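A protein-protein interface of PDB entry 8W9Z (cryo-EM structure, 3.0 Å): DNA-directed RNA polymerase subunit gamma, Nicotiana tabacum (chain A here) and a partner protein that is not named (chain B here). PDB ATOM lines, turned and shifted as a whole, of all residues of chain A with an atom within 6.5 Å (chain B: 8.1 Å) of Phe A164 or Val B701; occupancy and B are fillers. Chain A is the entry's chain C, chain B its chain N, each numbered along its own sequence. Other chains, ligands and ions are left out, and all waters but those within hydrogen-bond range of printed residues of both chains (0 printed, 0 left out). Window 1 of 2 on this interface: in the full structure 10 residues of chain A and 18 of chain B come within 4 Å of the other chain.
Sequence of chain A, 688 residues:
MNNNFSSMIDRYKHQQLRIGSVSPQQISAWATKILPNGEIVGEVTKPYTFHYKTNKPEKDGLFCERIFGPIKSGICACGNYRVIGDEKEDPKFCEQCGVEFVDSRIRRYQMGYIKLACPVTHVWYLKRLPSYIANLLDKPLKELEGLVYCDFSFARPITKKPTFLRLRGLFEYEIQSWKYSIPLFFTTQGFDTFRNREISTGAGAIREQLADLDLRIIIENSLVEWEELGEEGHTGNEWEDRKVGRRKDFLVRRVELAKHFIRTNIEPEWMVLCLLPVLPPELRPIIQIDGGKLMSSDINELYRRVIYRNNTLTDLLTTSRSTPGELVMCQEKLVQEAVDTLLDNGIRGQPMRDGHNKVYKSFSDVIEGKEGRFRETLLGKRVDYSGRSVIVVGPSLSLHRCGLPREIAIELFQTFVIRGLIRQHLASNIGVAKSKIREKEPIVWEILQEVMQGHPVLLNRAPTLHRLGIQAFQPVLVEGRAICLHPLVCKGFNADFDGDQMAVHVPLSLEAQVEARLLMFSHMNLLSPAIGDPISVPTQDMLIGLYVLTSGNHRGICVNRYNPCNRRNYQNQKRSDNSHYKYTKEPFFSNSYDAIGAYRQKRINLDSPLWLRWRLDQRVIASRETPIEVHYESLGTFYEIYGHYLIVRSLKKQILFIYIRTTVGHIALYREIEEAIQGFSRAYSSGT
Of chain B, only Val B701 (3.6 Å), Phe B762 (3.0 Å), Pro B763 (3.5 Å) and Trp B764 (2.9 Å) come within 4 Å of Phe A164. Val B701 touches two residues of chain A. Of the printed residues of chain A, Ala B745 touches Phe A185 (3.7 Å). Printed residues of chain B within 4 Å of Phe A185: Arg B704 (3.9 Å) and Ala B745 (3.7 Å). Of the printed residues of chain A, Arg B700 touches Phe A186 (2.4 Å). Of the printed residues of chain A, Trp B764 touches Phe A164 (2.9 Å), Arg A166 (3.2 Å) and Phe A186 (3.6 Å). Of the printed residues of chain B, Thr A163 touches Tyr B684 (3.8 Å) and Phe B762 (3.2 Å). The nearest residue of chain A that does not touch Val B701 is Phe A194 (5.0 Å).
O of Leu B695 touches CB of Pro A162, at 3.5 Å. OH of Tyr B684 touches O of Thr A163, 3.8 Å away. CE2 of Phe B762 touches O of Thr A163 (3.2 Å). Phe A164 touches Val B701. Phe A164 touches Pro B763. Leu B766 touches Arg A166. Phe A185 touches Arg B704 (CE2 to CB, 3.9 Å). Phe A185 touches Ala B745. Phe A186 touches Arg B704. Phe A186 touches Trp B764 (CZ to CH2, 3.6 Å).
A ring nitrogen (NE2) of His B696 sits close to the backbone carbonyl oxygen (O) of Pro A162 (3.5 Å). O of Phe A186 is in hydrogen-bond range of NE of Arg B700 (3.0 Å). The backbone carbonyl oxygen (O) of Phe A164 is in hydrogen-bond range of the backbone NH (N) of Trp B764 (2.9 Å). The backbone carbonyl oxygen (O) of Trp B764 is in hydrogen-bond range of the backbone NH (N) of Arg A166, 3.2 Å away. O of Phe A164 lies close to O of Phe B762 (3.0 Å).
ND1 of His B696 lies within hydrogen-bond range of N of Ile B698 (3.1 Å). The backbone carbonyl oxygen (O) of Glu B761 sits close to the indole nitrogen (NE1) of Trp B764 (3.4 Å).
Of the 12 printed residues of chain A, 6 touch a printed residue of chain B. Printed residues of chain A that touch a printed residue of chain B: Pro A162, Thr A163, Phe A164, Arg A166, Phe A185 and Phe A186. Hydrophobic or aromatic side chains of chain A within 4 Å of the printed part of chain B: Pro A162, Phe A164, Phe A185 and Phe A186. Hydrophobic or aromatic side chains of chain B that line the printed part of chain A: Tyr B684, His B696, Val B701, Phe B762 and Trp B764. Among the printed residues, 16 pairs touch across the chains. Among the printed residues, no Asp or Glu carboxylate lies within 4 Å of a Lys or Arg side-chain nitrogen of the other chain.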
ATOM      1  N   PRO A 162      27.613 -10.425  18.531  1.00  0.00           N
ATOM      2  CA  PRO A 162      27.214  -9.805  19.802  1.00  0.00           C
ATOM      3  C   PRO A 162      27.924 -10.454  20.981  1.00  0.00           C
ATOM      4  O   PRO A 162      27.941 -11.679  21.124  1.00  0.00           O
ATOM      5  CB  PRO A 162      25.699 -10.037  19.850  1.00  0.00           C
ATOM      6  CG  PRO A 162      25.460 -11.191  18.931  1.00  0.00           C
ATOM      7  CD  PRO A 162      26.473 -11.051  17.840  1.00  0.00           C
ATOM      8  N   THR A 163      28.513  -9.615  21.829  1.00  0.00           N
ATOM      9  CA  THR A 163      29.276 -10.060  22.986  1.00  0.00           C
ATOM     10  C   THR A 163      28.553  -9.656  24.262  1.00  0.00           C
ATOM     11  O   THR A 163      27.914  -8.601  24.318  1.00  0.00           O
ATOM     12  CB  THR A 163      30.691  -9.469  22.980  1.00  0.00           C
ATOM     13  OG1 THR A 163      30.617  -8.042  23.087  1.00  0.00           O
ATOM     14  CG2 THR A 163      31.415  -9.838  21.694  1.00  0.00           C
ATOM     15  N   PHE A 164      28.661 -10.502  25.287  1.00  0.00           N
ATOM     16  CA  PHE A 164      27.998 -10.268  26.560  1.00  0.00           C
ATOM     17  C   PHE A 164      28.966 -10.129  27.724  1.00  0.00           C
ATOM     18  O   PHE A 164      28.527  -9.846  28.845  1.00  0.00           O
ATOM     19  CB  PHE A 164      27.004 -11.400  26.858  1.00  0.00           C
ATOM     20  CG  PHE A 164      27.656 -12.711  27.187  1.00  0.00           C
ATOM     21  CD1 PHE A 164      28.216 -13.493  26.191  1.00  0.00           C
ATOM     22  CD2 PHE A 164      27.701 -13.167  28.494  1.00  0.00           C
ATOM     23  CE1 PHE A 164      28.817 -14.700  26.493  1.00  0.00           C
ATOM     24  CE2 PHE A 164      28.297 -14.373  28.802  1.00  0.00           C
ATOM     25  CZ  PHE A 164      28.856 -15.141  27.801  1.00  0.00           C
ATOM     26  N   LEU A 165      30.264 -10.315  27.498  1.00  0.00           N
ATOM     27  CA  LEU A 165      31.272 -10.207  28.549  1.00  0.00           C
ATOM     28  C   LEU A 165      31.826  -8.787  28.527  1.00  0.00           C
ATOM     29  O   LEU A 165      32.658  -8.445  27.683  1.00  0.00           O
ATOM     30  CB  LEU A 165      32.375 -11.242  28.349  1.00  0.00           C
ATOM     31  CG  LEU A 165      31.961 -12.712  28.443  1.00  0.00           C
ATOM     32  CD1 LEU A 165      33.128 -13.622  28.099  1.00  0.00           C
ATOM     33  CD2 LEU A 165      31.425 -13.027  29.830  1.00  0.00           C
ATOM     34  N   ARG A 166      31.361  -7.959  29.460  1.00  0.00           N
ATOM     35  CA  ARG A 166      31.801  -6.570  29.561  1.00  0.00           C
ATOM     36  C   ARG A 166      33.094  -6.545  30.367  1.00  0.00           C
ATOM     37  O   ARG A 166      33.075  -6.604  31.599  1.00  0.00           O
ATOM     38  CB  ARG A 166      30.716  -5.707  30.197  1.00  0.00           C
ATOM     39  CG  ARG A 166      30.939  -4.201  30.073  1.00  0.00           C
ATOM     40  CD  ARG A 166      31.767  -3.649  31.225  1.00  0.00           C
ATOM     41  NE  ARG A 166      32.008  -2.215  31.091  1.00  0.00           N
ATOM     42  CZ  ARG A 166      32.713  -1.493  31.955  1.00  0.00           C
ATOM     43  NH1 ARG A 166      32.880  -0.192  31.753  1.00  0.00           N
ATOM     44  NH2 ARG A 166      33.251  -2.068  33.022  1.00  0.00           N
ATOM     45  N   ILE A 182      33.175 -19.701  35.089  1.00  0.00           N
ATOM     46  CA  ILE A 182      32.519 -19.269  33.856  1.00  0.00           C
ATOM     47  C   ILE A 182      32.587 -20.396  32.831  1.00  0.00           C
ATOM     48  O   ILE A 182      31.577 -20.699  32.177  1.00  0.00           O
ATOM     49  CB  ILE A 182      33.147 -17.973  33.314  1.00  0.00           C
ATOM     50  CG1 ILE A 182      32.447 -16.743  33.904  1.00  0.00           C
ATOM     51  CG2 ILE A 182      33.085 -17.929  31.792  1.00  0.00           C
ATOM     52  CD1 ILE A 182      32.657 -16.547  35.391  1.00  0.00           C
ATOM     53  N   PHE A 185      30.269 -23.317  33.738  1.00  0.00           N
ATOM     54  CA  PHE A 185      28.865 -22.976  33.945  1.00  0.00           C
ATOM     55  C   PHE A 185      28.000 -23.457  32.787  1.00  0.00           C
ATOM     56  O   PHE A 185      27.106 -24.291  32.968  1.00  0.00           O
ATOM     57  CB  PHE A 185      28.711 -21.466  34.136  1.00  0.00           C
ATOM     58  CG  PHE A 185      27.308 -20.974  33.928  1.00  0.00           C
ATOM     59  CD1 PHE A 185      26.295 -21.346  34.795  1.00  0.00           C
ATOM     60  CD2 PHE A 185      27.000 -20.142  32.865  1.00  0.00           C
ATOM     61  CE1 PHE A 185      25.001 -20.900  34.607  1.00  0.00           C
ATOM     62  CE2 PHE A 185      25.708 -19.691  32.673  1.00  0.00           C
ATOM     63  CZ  PHE A 185      24.708 -20.071  33.544  1.00  0.00           C
ATOM     64  N   PHE A 186      28.244 -22.931  31.586  1.00  0.00           N
ATOM     65  CA  PHE A 186      27.375 -23.195  30.446  1.00  0.00           C
ATOM     66  C   PHE A 186      27.350 -24.673  30.079  1.00  0.00           C
ATOM     67  O   PHE A 186      26.311 -25.329  30.209  1.00  0.00           O
ATOM     68  CB  PHE A 186      27.817 -22.369  29.236  1.00  0.00           C
ATOM     69  CG  PHE A 186      27.870 -20.891  29.497  1.00  0.00           C
ATOM     70  CD1 PHE A 186      26.749 -20.101  29.314  1.00  0.00           C
ATOM     71  CD2 PHE A 186      29.045 -20.290  29.917  1.00  0.00           C
ATOM     72  CE1 PHE A 186      26.795 -18.740  29.552  1.00  0.00           C
ATOM     73  CE2 PHE A 186      29.099 -18.930  30.156  1.00  0.00           C
ATOM     74  CZ  PHE A 186      27.972 -18.153  29.972  1.00  0.00           C
ATOM     75  N   GLY A 190      31.014 -25.849  25.269  1.00  0.00           N
ATOM     76  CA  GLY A 190      30.165 -24.691  25.075  1.00  0.00           C
ATOM     77  C   GLY A 190      30.921 -23.407  25.345  1.00  0.00           C
ATOM     78  O   GLY A 190      30.548 -22.336  24.861  1.00  0.00           O
ATOM     79  N   THR A 193      33.332 -22.493  21.990  1.00  0.00           N
ATOM     80  CA  THR A 193      32.722 -21.918  20.797  1.00  0.00           C
ATOM     81  C   THR A 193      32.556 -20.405  20.884  1.00  0.00           C
ATOM     82  O   THR A 193      32.355 -19.761  19.850  1.00  0.00           O
ATOM     83  CB  THR A 193      31.362 -22.567  20.529  1.00  0.00           C
ATOM     84  OG1 THR A 193      30.822 -22.058  19.303  1.00  0.00           O
ATOM     85  CG2 THR A 193      30.394 -22.269  21.662  1.00  0.00           C
ATOM     86  N   PHE A 194      32.632 -19.823  22.083  1.00  0.00           N
ATOM     87  CA  PHE A 194      32.483 -18.383  22.236  1.00  0.00           C
ATOM     88  C   PHE A 194      33.661 -17.706  22.923  1.00  0.00           C
ATOM     89  O   PHE A 194      33.682 -16.472  22.989  1.00  0.00           O
ATOM     90  CB  PHE A 194      31.195 -18.053  23.010  1.00  0.00           C
ATOM     91  CG  PHE A 194      31.373 -17.995  24.501  1.00  0.00           C
ATOM     92  CD1 PHE A 194      31.433 -19.155  25.252  1.00  0.00           C
ATOM     93  CD2 PHE A 194      31.463 -16.775  25.154  1.00  0.00           C
ATOM     94  CE1 PHE A 194      31.591 -19.101  26.625  1.00  0.00           C
ATOM     95  CE2 PHE A 194      31.626 -16.716  26.524  1.00  0.00           C
ATOM     96  CZ  PHE A 194      31.688 -17.880  27.261  1.00  0.00           C
ATOM     97  N   GLU A 198      35.971 -13.031  22.860  1.00  0.00           N
ATOM     98  CA  GLU A 198      36.427 -12.115  23.897  1.00  0.00           C
ATOM     99  C   GLU A 198      37.821 -12.445  24.409  1.00  0.00           C
ATOM    100  O   GLU A 198      38.687 -11.566  24.458  1.00  0.00           O
ATOM    101  CB  GLU A 198      35.434 -12.106  25.071  1.00  0.00           C
ATOM    102  CG  GLU A 198      34.038 -11.612  24.720  1.00  0.00           C
ATOM    103  CD  GLU A 198      33.175 -12.685  24.085  1.00  0.00           C
ATOM    104  OE1 GLU A 198      33.651 -13.832  23.955  1.00  0.00           O
ATOM    105  OE2 GLU A 198      32.021 -12.383  23.720  1.00  0.00           O
ATOM    106  N   VAL B 619      13.138 -16.135  24.810  1.00  0.00           N
ATOM    107  CA  VAL B 619      14.243 -16.335  23.880  1.00  0.00           C
ATOM    108  C   VAL B 619      13.787 -17.309  22.804  1.00  0.00           C
ATOM    109  O   VAL B 619      13.273 -18.389  23.114  1.00  0.00           O
ATOM    110  CB  VAL B 619      15.512 -16.850  24.591  1.00  0.00           C
ATOM    111  CG1 VAL B 619      15.166 -17.961  25.574  1.00  0.00           C
ATOM    112  CG2 VAL B 619      16.538 -17.329  23.575  1.00  0.00           C
ATOM    113  N   THR B 648      17.856 -15.391  18.909  1.00  0.00           N
ATOM    114  CA  THR B 648      18.930 -16.296  18.522  1.00  0.00           C
ATOM    115  C   THR B 648      18.614 -16.975  17.195  1.00  0.00           C
ATOM    116  O   THR B 648      17.656 -16.602  16.512  1.00  0.00           O
ATOM    117  CB  THR B 648      19.167 -17.354  19.603  1.00  0.00           C
ATOM    118  OG1 THR B 648      17.957 -18.087  19.828  1.00  0.00           O
ATOM    119  CG2 THR B 648      19.609 -16.703  20.902  1.00  0.00           C
ATOM    120  N   GLY B 679      27.371  -1.858  21.051  1.00  0.00           N
ATOM    121  CA  GLY B 679      28.029  -2.828  21.907  1.00  0.00           C
ATOM    122  C   GLY B 679      29.463  -2.483  22.244  1.00  0.00           C
ATOM    123  O   GLY B 679      29.966  -2.924  23.283  1.00  0.00           O
ATOM    124  N   TYR B 684      23.855   0.525  25.641  1.00  0.00           N
ATOM    125  CA  TYR B 684      22.771  -0.308  25.126  1.00  0.00           C
ATOM    126  C   TYR B 684      21.421   0.371  25.337  1.00  0.00           C
ATOM    127  O   TYR B 684      20.669  -0.015  26.241  1.00  0.00           O
ATOM    128  CB  TYR B 684      22.785  -1.687  25.787  1.00  0.00           C
ATOM    129  CG  TYR B 684      23.979  -2.533  25.409  1.00  0.00           C
ATOM    130  CD1 TYR B 684      25.170  -2.446  26.116  1.00  0.00           C
ATOM    131  CD2 TYR B 684      23.913  -3.421  24.344  1.00  0.00           C
ATOM    132  CE1 TYR B 684      26.263  -3.219  25.774  1.00  0.00           C
ATOM    133  CE2 TYR B 684      25.000  -4.198  23.993  1.00  0.00           C
ATOM    134  CZ  TYR B 684      26.173  -4.093  24.711  1.00  0.00           C
ATOM    135  OH  TYR B 684      27.258  -4.865  24.366  1.00  0.00           O
ATOM    136  N   PHE B 694      17.735  -8.078  23.490  1.00  0.00           N
ATOM    137  CA  PHE B 694      19.076  -8.635  23.399  1.00  0.00           C
ATOM    138  C   PHE B 694      19.125  -9.655  22.269  1.00  0.00           C
ATOM    139  O   PHE B 694      18.098 -10.062  21.720  1.00  0.00           O
ATOM    140  CB  PHE B 694      19.498  -9.288  24.722  1.00  0.00           C
ATOM    141  CG  PHE B 694      19.609  -8.324  25.868  1.00  0.00           C
ATOM    142  CD1 PHE B 694      20.027  -7.022  25.659  1.00  0.00           C
ATOM    143  CD2 PHE B 694      19.294  -8.722  27.157  1.00  0.00           C
ATOM    144  CE1 PHE B 694      20.131  -6.133  26.713  1.00  0.00           C
ATOM    145  CE2 PHE B 694      19.395  -7.839  28.215  1.00  0.00           C
ATOM    146  CZ  PHE B 694      19.815  -6.543  27.993  1.00  0.00           C
ATOM    147  N   LEU B 695      20.342 -10.067  21.920  1.00  0.00           N
ATOM    148  CA  LEU B 695      20.528 -11.060  20.872  1.00  0.00           C
ATOM    149  C   LEU B 695      21.898 -11.702  21.028  1.00  0.00           C
ATOM    150  O   LEU B 695      22.826 -11.094  21.570  1.00  0.00           O
ATOM    151  CB  LEU B 695      20.390 -10.447  19.470  1.00  0.00           C
ATOM    152  CG  LEU B 695      21.605  -9.726  18.876  1.00  0.00           C
ATOM    153  CD1 LEU B 695      21.390  -9.446  17.397  1.00  0.00           C
ATOM    154  CD2 LEU B 695      21.905  -8.436  19.620  1.00  0.00           C
ATOM    155  N   HIS B 696      22.009 -12.939  20.551  1.00  0.00           N
ATOM    156  CA  HIS B 696      23.284 -13.639  20.515  1.00  0.00           C
ATOM    157  C   HIS B 696      23.222 -14.705  19.431  1.00  0.00           C
ATOM    158  O   HIS B 696      22.146 -15.204  19.091  1.00  0.00           O
ATOM    159  CB  HIS B 696      23.632 -14.270  21.866  1.00  0.00           C
ATOM    160  CG  HIS B 696      25.069 -14.672  21.989  1.00  0.00           C
ATOM    161  ND1 HIS B 696      25.556 -15.862  21.493  1.00  0.00           N
ATOM    162  CD2 HIS B 696      26.126 -14.038  22.551  1.00  0.00           C
ATOM    163  CE1 HIS B 696      26.851 -15.944  21.743  1.00  0.00           C
ATOM    164  NE2 HIS B 696      27.221 -14.851  22.385  1.00  0.00           N
ATOM    165  N   ASP B 697      24.392 -15.046  18.889  1.00  0.00           N
ATOM    166  CA  ASP B 697      24.453 -16.015  17.800  1.00  0.00           C
ATOM    167  C   ASP B 697      24.216 -17.432  18.311  1.00  0.00           C
ATOM    168  O   ASP B 697      23.288 -18.119  17.869  1.00  0.00           O
ATOM    169  CB  ASP B 697      25.803 -15.915  17.086  1.00  0.00           C
ATOM    170  N   ILE B 698      25.050 -17.888  19.247  1.00  0.00           N
ATOM    171  CA  ILE B 698      24.945 -19.253  19.744  1.00  0.00           C
ATOM    172  C   ILE B 698      23.707 -19.391  20.621  1.00  0.00           C
ATOM    173  O   ILE B 698      23.292 -18.442  21.300  1.00  0.00           O
ATOM    174  CB  ILE B 698      26.218 -19.647  20.511  1.00  0.00           C
ATOM    175  N   ARG B 699      23.111 -20.585  20.609  1.00  0.00           N
ATOM    176  CA  ARG B 699      21.872 -20.808  21.345  1.00  0.00           C
ATOM    177  C   ARG B 699      22.132 -21.190  22.798  1.00  0.00           C
ATOM    178  O   ARG B 699      21.391 -20.769  23.692  1.00  0.00           O
ATOM    179  CB  ARG B 699      21.042 -21.891  20.656  1.00  0.00           C
ATOM    180  N   ARG B 700      23.177 -21.981  23.052  1.00  0.00           N
ATOM    181  CA  ARG B 700      23.406 -22.506  24.396  1.00  0.00           C
ATOM    182  C   ARG B 700      23.735 -21.390  25.383  1.00  0.00           C
ATOM    183  O   ARG B 700      23.132 -21.306  26.461  1.00  0.00           O
ATOM    184  CB  ARG B 700      24.524 -23.551  24.364  1.00  0.00           C
ATOM    185  CG  ARG B 700      25.053 -23.950  25.737  1.00  0.00           C
ATOM    186  CD  ARG B 700      23.943 -24.440  26.656  1.00  0.00           C
ATOM    187  NE  ARG B 700      24.393 -24.537  28.042  1.00  0.00           N
ATOM    188  CZ  ARG B 700      23.586 -24.470  29.095  1.00  0.00           C
ATOM    189  NH1 ARG B 700      22.283 -24.294  28.922  1.00  0.00           N
ATOM    190  NH2 ARG B 700      24.082 -24.567  30.320  1.00  0.00           N
ATOM    191  N   VAL B 701      24.697 -20.533  25.040  1.00  0.00           N
ATOM    192  CA  VAL B 701      25.112 -19.479  25.962  1.00  0.00           C
ATOM    193  C   VAL B 701      23.972 -18.495  26.197  1.00  0.00           C
ATOM    194  O   VAL B 701      23.738 -18.055  27.330  1.00  0.00           O
ATOM    195  CB  VAL B 701      26.378 -18.778  25.433  1.00  0.00           C
ATOM    196  CG1 VAL B 701      26.237 -18.468  23.955  1.00  0.00           C
ATOM    197  CG2 VAL B 701      26.656 -17.508  26.221  1.00  0.00           C
ATOM    198  N   ALA B 702      23.232 -18.153  25.141  1.00  0.00           N
ATOM    199  CA  ALA B 702      22.126 -17.214  25.291  1.00  0.00           C
ATOM    200  C   ALA B 702      21.004 -17.808  26.133  1.00  0.00           C
ATOM    201  O   ALA B 702      20.402 -17.107  26.956  1.00  0.00           O
ATOM    202  CB  ALA B 702      21.604 -16.794  23.917  1.00  0.00           C
ATOM    203  N   VAL B 703      20.715 -19.098  25.952  1.00  0.00           N
ATOM    204  CA  VAL B 703      19.676 -19.741  26.750  1.00  0.00           C
ATOM    205  C   VAL B 703      20.097 -19.821  28.211  1.00  0.00           C
ATOM    206  O   VAL B 703      19.286 -19.597  29.118  1.00  0.00           O
ATOM    207  CB  VAL B 703      19.348 -21.132  26.178  1.00  0.00           C
ATOM    208  N   ARG B 704      21.370 -20.134  28.466  1.00  0.00           N
ATOM    209  CA  ARG B 704      21.854 -20.179  29.841  1.00  0.00           C
ATOM    210  C   ARG B 704      21.806 -18.798  30.484  1.00  0.00           C
ATOM    211  O   ARG B 704      21.480 -18.667  31.669  1.00  0.00           O
ATOM    212  CB  ARG B 704      23.274 -20.742  29.881  1.00  0.00           C
ATOM    213  N   CYS B 705      22.118 -17.754  29.713  1.00  0.00           N
ATOM    214  CA  CYS B 705      22.036 -16.398  30.242  1.00  0.00           C
ATOM    215  C   CYS B 705      20.595 -16.013  30.550  1.00  0.00           C
ATOM    216  O   CYS B 705      20.317 -15.417  31.596  1.00  0.00           O
ATOM    217  CB  CYS B 705      22.656 -15.411  29.254  1.00  0.00           C
ATOM    218  N   ALA B 706      19.665 -16.349  29.651  1.00  0.00           N
ATOM    219  CA  ALA B 706      18.259 -16.044  29.891  1.00  0.00           C
ATOM    220  C   ALA B 706      17.734 -16.790  31.110  1.00  0.00           C
ATOM    221  O   ALA B 706      16.930 -16.250  31.879  1.00  0.00           O
ATOM    222  CB  ALA B 706      17.430 -16.384  28.652  1.00  0.00           C
ATOM    223  N   VAL B 707      18.176 -18.035  31.302  1.00  0.00           N
ATOM    224  CA  VAL B 707      17.795 -18.771  32.503  1.00  0.00           C
ATOM    225  C   VAL B 707      18.430 -18.149  33.738  1.00  0.00           C
ATOM    226  O   VAL B 707      17.860 -18.204  34.834  1.00  0.00           O
ATOM    227  CB  VAL B 707      18.173 -20.257  32.362  1.00  0.00           C
ATOM    228  N   ALA B 708      19.613 -17.549  33.588  1.00  0.00           N
ATOM    229  CA  ALA B 708      20.275 -16.911  34.720  1.00  0.00           C
ATOM    230  C   ALA B 708      19.804 -15.477  34.927  1.00  0.00           C
ATOM    231  O   ALA B 708      19.815 -14.985  36.061  1.00  0.00           O
ATOM    232  CB  ALA B 708      21.791 -16.942  34.529  1.00  0.00           C
ATOM    233  N   ALA B 745      21.891 -24.974  34.394  1.00  0.00           N
ATOM    234  CA  ALA B 745      22.078 -23.532  34.526  1.00  0.00           C
ATOM    235  C   ALA B 745      21.462 -23.009  35.817  1.00  0.00           C
ATOM    236  O   ALA B 745      22.069 -22.183  36.511  1.00  0.00           O
ATOM    237  CB  ALA B 745      21.485 -22.813  33.315  1.00  0.00           C
ATOM    238  N   ASP B 758      27.570 -10.535  37.648  1.00  0.00           N
ATOM    239  CA  ASP B 758      26.291  -9.845  37.543  1.00  0.00           C
ATOM    240  C   ASP B 758      25.570 -10.329  36.292  1.00  0.00           C
ATOM    241  O   ASP B 758      26.093 -10.201  35.179  1.00  0.00           O
ATOM    242  CB  ASP B 758      26.492  -8.331  37.500  1.00  0.00           C
ATOM    243  CG  ASP B 758      25.181  -7.564  37.515  1.00  0.00           C
ATOM    244  OD1 ASP B 758      24.122  -8.185  37.742  1.00  0.00           O
ATOM    245  OD2 ASP B 758      25.212  -6.334  37.300  1.00  0.00           O
ATOM    246  N   THR B 759      24.372 -10.883  36.476  1.00  0.00           N
ATOM    247  CA  THR B 759      23.547 -11.368  35.376  1.00  0.00           C
ATOM    248  C   THR B 759      22.241 -10.584  35.265  1.00  0.00           C
ATOM    249  O   THR B 759      21.194 -11.146  34.935  1.00  0.00           O
ATOM    250  CB  THR B 759      23.266 -12.861  35.538  1.00  0.00           C
ATOM    251  OG1 THR B 759      24.380 -13.486  36.186  1.00  0.00           O
ATOM    252  CG2 THR B 759      23.062 -13.516  34.178  1.00  0.00           C
ATOM    253  N   GLU B 761      21.689  -7.855  33.186  1.00  0.00           N
ATOM    254  CA  GLU B 761      21.467  -7.531  31.784  1.00  0.00           C
ATOM    255  C   GLU B 761      22.410  -8.360  30.920  1.00  0.00           C
ATOM    256  O   GLU B 761      23.143  -9.225  31.411  1.00  0.00           O
ATOM    257  CB  GLU B 761      21.661  -6.031  31.525  1.00  0.00           C
ATOM    258  N   PHE B 762      22.383  -8.091  29.616  1.00  0.00           N
ATOM    259  CA  PHE B 762      23.261  -8.803  28.689  1.00  0.00           C
ATOM    260  C   PHE B 762      24.736  -8.494  28.920  1.00  0.00           C
ATOM    261  O   PHE B 762      25.544  -9.439  28.937  1.00  0.00           O
ATOM    262  CB  PHE B 762      22.836  -8.498  27.249  1.00  0.00           C
ATOM    263  CG  PHE B 762      23.427  -9.427  26.228  1.00  0.00           C
ATOM    264  CD1 PHE B 762      22.963 -10.726  26.104  1.00  0.00           C
ATOM    265  CD2 PHE B 762      24.435  -8.997  25.381  1.00  0.00           C
ATOM    266  CE1 PHE B 762      23.499 -11.583  25.162  1.00  0.00           C
ATOM    267  CE2 PHE B 762      24.974  -9.849  24.436  1.00  0.00           C
ATOM    268  CZ  PHE B 762      24.507 -11.143  24.327  1.00  0.00           C
ATOM    269  N   PRO B 763      25.167  -7.229  29.105  1.00  0.00           N
ATOM    270  CA  PRO B 763      26.586  -6.988  29.405  1.00  0.00           C
ATOM    271  C   PRO B 763      26.948  -7.336  30.840  1.00  0.00           C
ATOM    272  O   PRO B 763      26.927  -6.468  31.719  1.00  0.00           O
ATOM    273  CB  PRO B 763      26.752  -5.489  29.129  1.00  0.00           C
ATOM    274  CG  PRO B 763      25.411  -4.920  29.384  1.00  0.00           C
ATOM    275  CD  PRO B 763      24.436  -5.960  28.916  1.00  0.00           C
ATOM    276  N   TRP B 764      27.263  -8.608  31.089  1.00  0.00           N
ATOM    277  CA  TRP B 764      27.640  -9.047  32.429  1.00  0.00           C
ATOM    278  C   TRP B 764      28.832  -8.251  32.942  1.00  0.00           C
ATOM    279  O   TRP B 764      29.863  -8.147  32.270  1.00  0.00           O
ATOM    280  CB  TRP B 764      27.976 -10.539  32.427  1.00  0.00           C
ATOM    281  CG  TRP B 764      26.831 -11.442  32.085  1.00  0.00           C
ATOM    282  CD1 TRP B 764      25.557 -11.072  31.766  1.00  0.00           C
ATOM    283  CD2 TRP B 764      26.858 -12.872  32.028  1.00  0.00           C
ATOM    284  NE1 TRP B 764      24.790 -12.183  31.514  1.00  0.00           N
ATOM    285  CE2 TRP B 764      25.565 -13.301  31.668  1.00  0.00           C
ATOM    286  CE3 TRP B 764      27.850 -13.833  32.247  1.00  0.00           C
ATOM    287  CZ2 TRP B 764      25.239 -14.648  31.521  1.00  0.00           C
ATOM    288  CZ3 TRP B 764      27.523 -15.170  32.101  1.00  0.00           C
ATOM    289  CH2 TRP B 764      26.229 -15.565  31.741  1.00  0.00           C
ATOM    290  N   ARG B 765      28.687  -7.685  34.137  1.00  0.00           N
ATOM    291  CA  ARG B 765      29.759  -6.921  34.769  1.00  0.00           C
ATOM    292  C   ARG B 765      30.742  -7.904  35.390  1.00  0.00           C
ATOM    293  O   ARG B 765      30.496  -8.456  36.465  1.00  0.00           O
ATOM    294  CB  ARG B 765      29.189  -5.961  35.809  1.00  0.00           C
ATOM    295  N   LEU B 766      31.861  -8.132  34.709  1.00  0.00           N
ATOM    296  CA  LEU B 766      32.871  -9.056  35.215  1.00  0.00           C
ATOM    297  C   LEU B 766      33.843  -8.320  36.128  1.00  0.00           C
ATOM    298  O   LEU B 766      34.387  -7.283  35.732  1.00  0.00           O
ATOM    299  CB  LEU B 766      33.636  -9.710  34.071  1.00  0.00           C
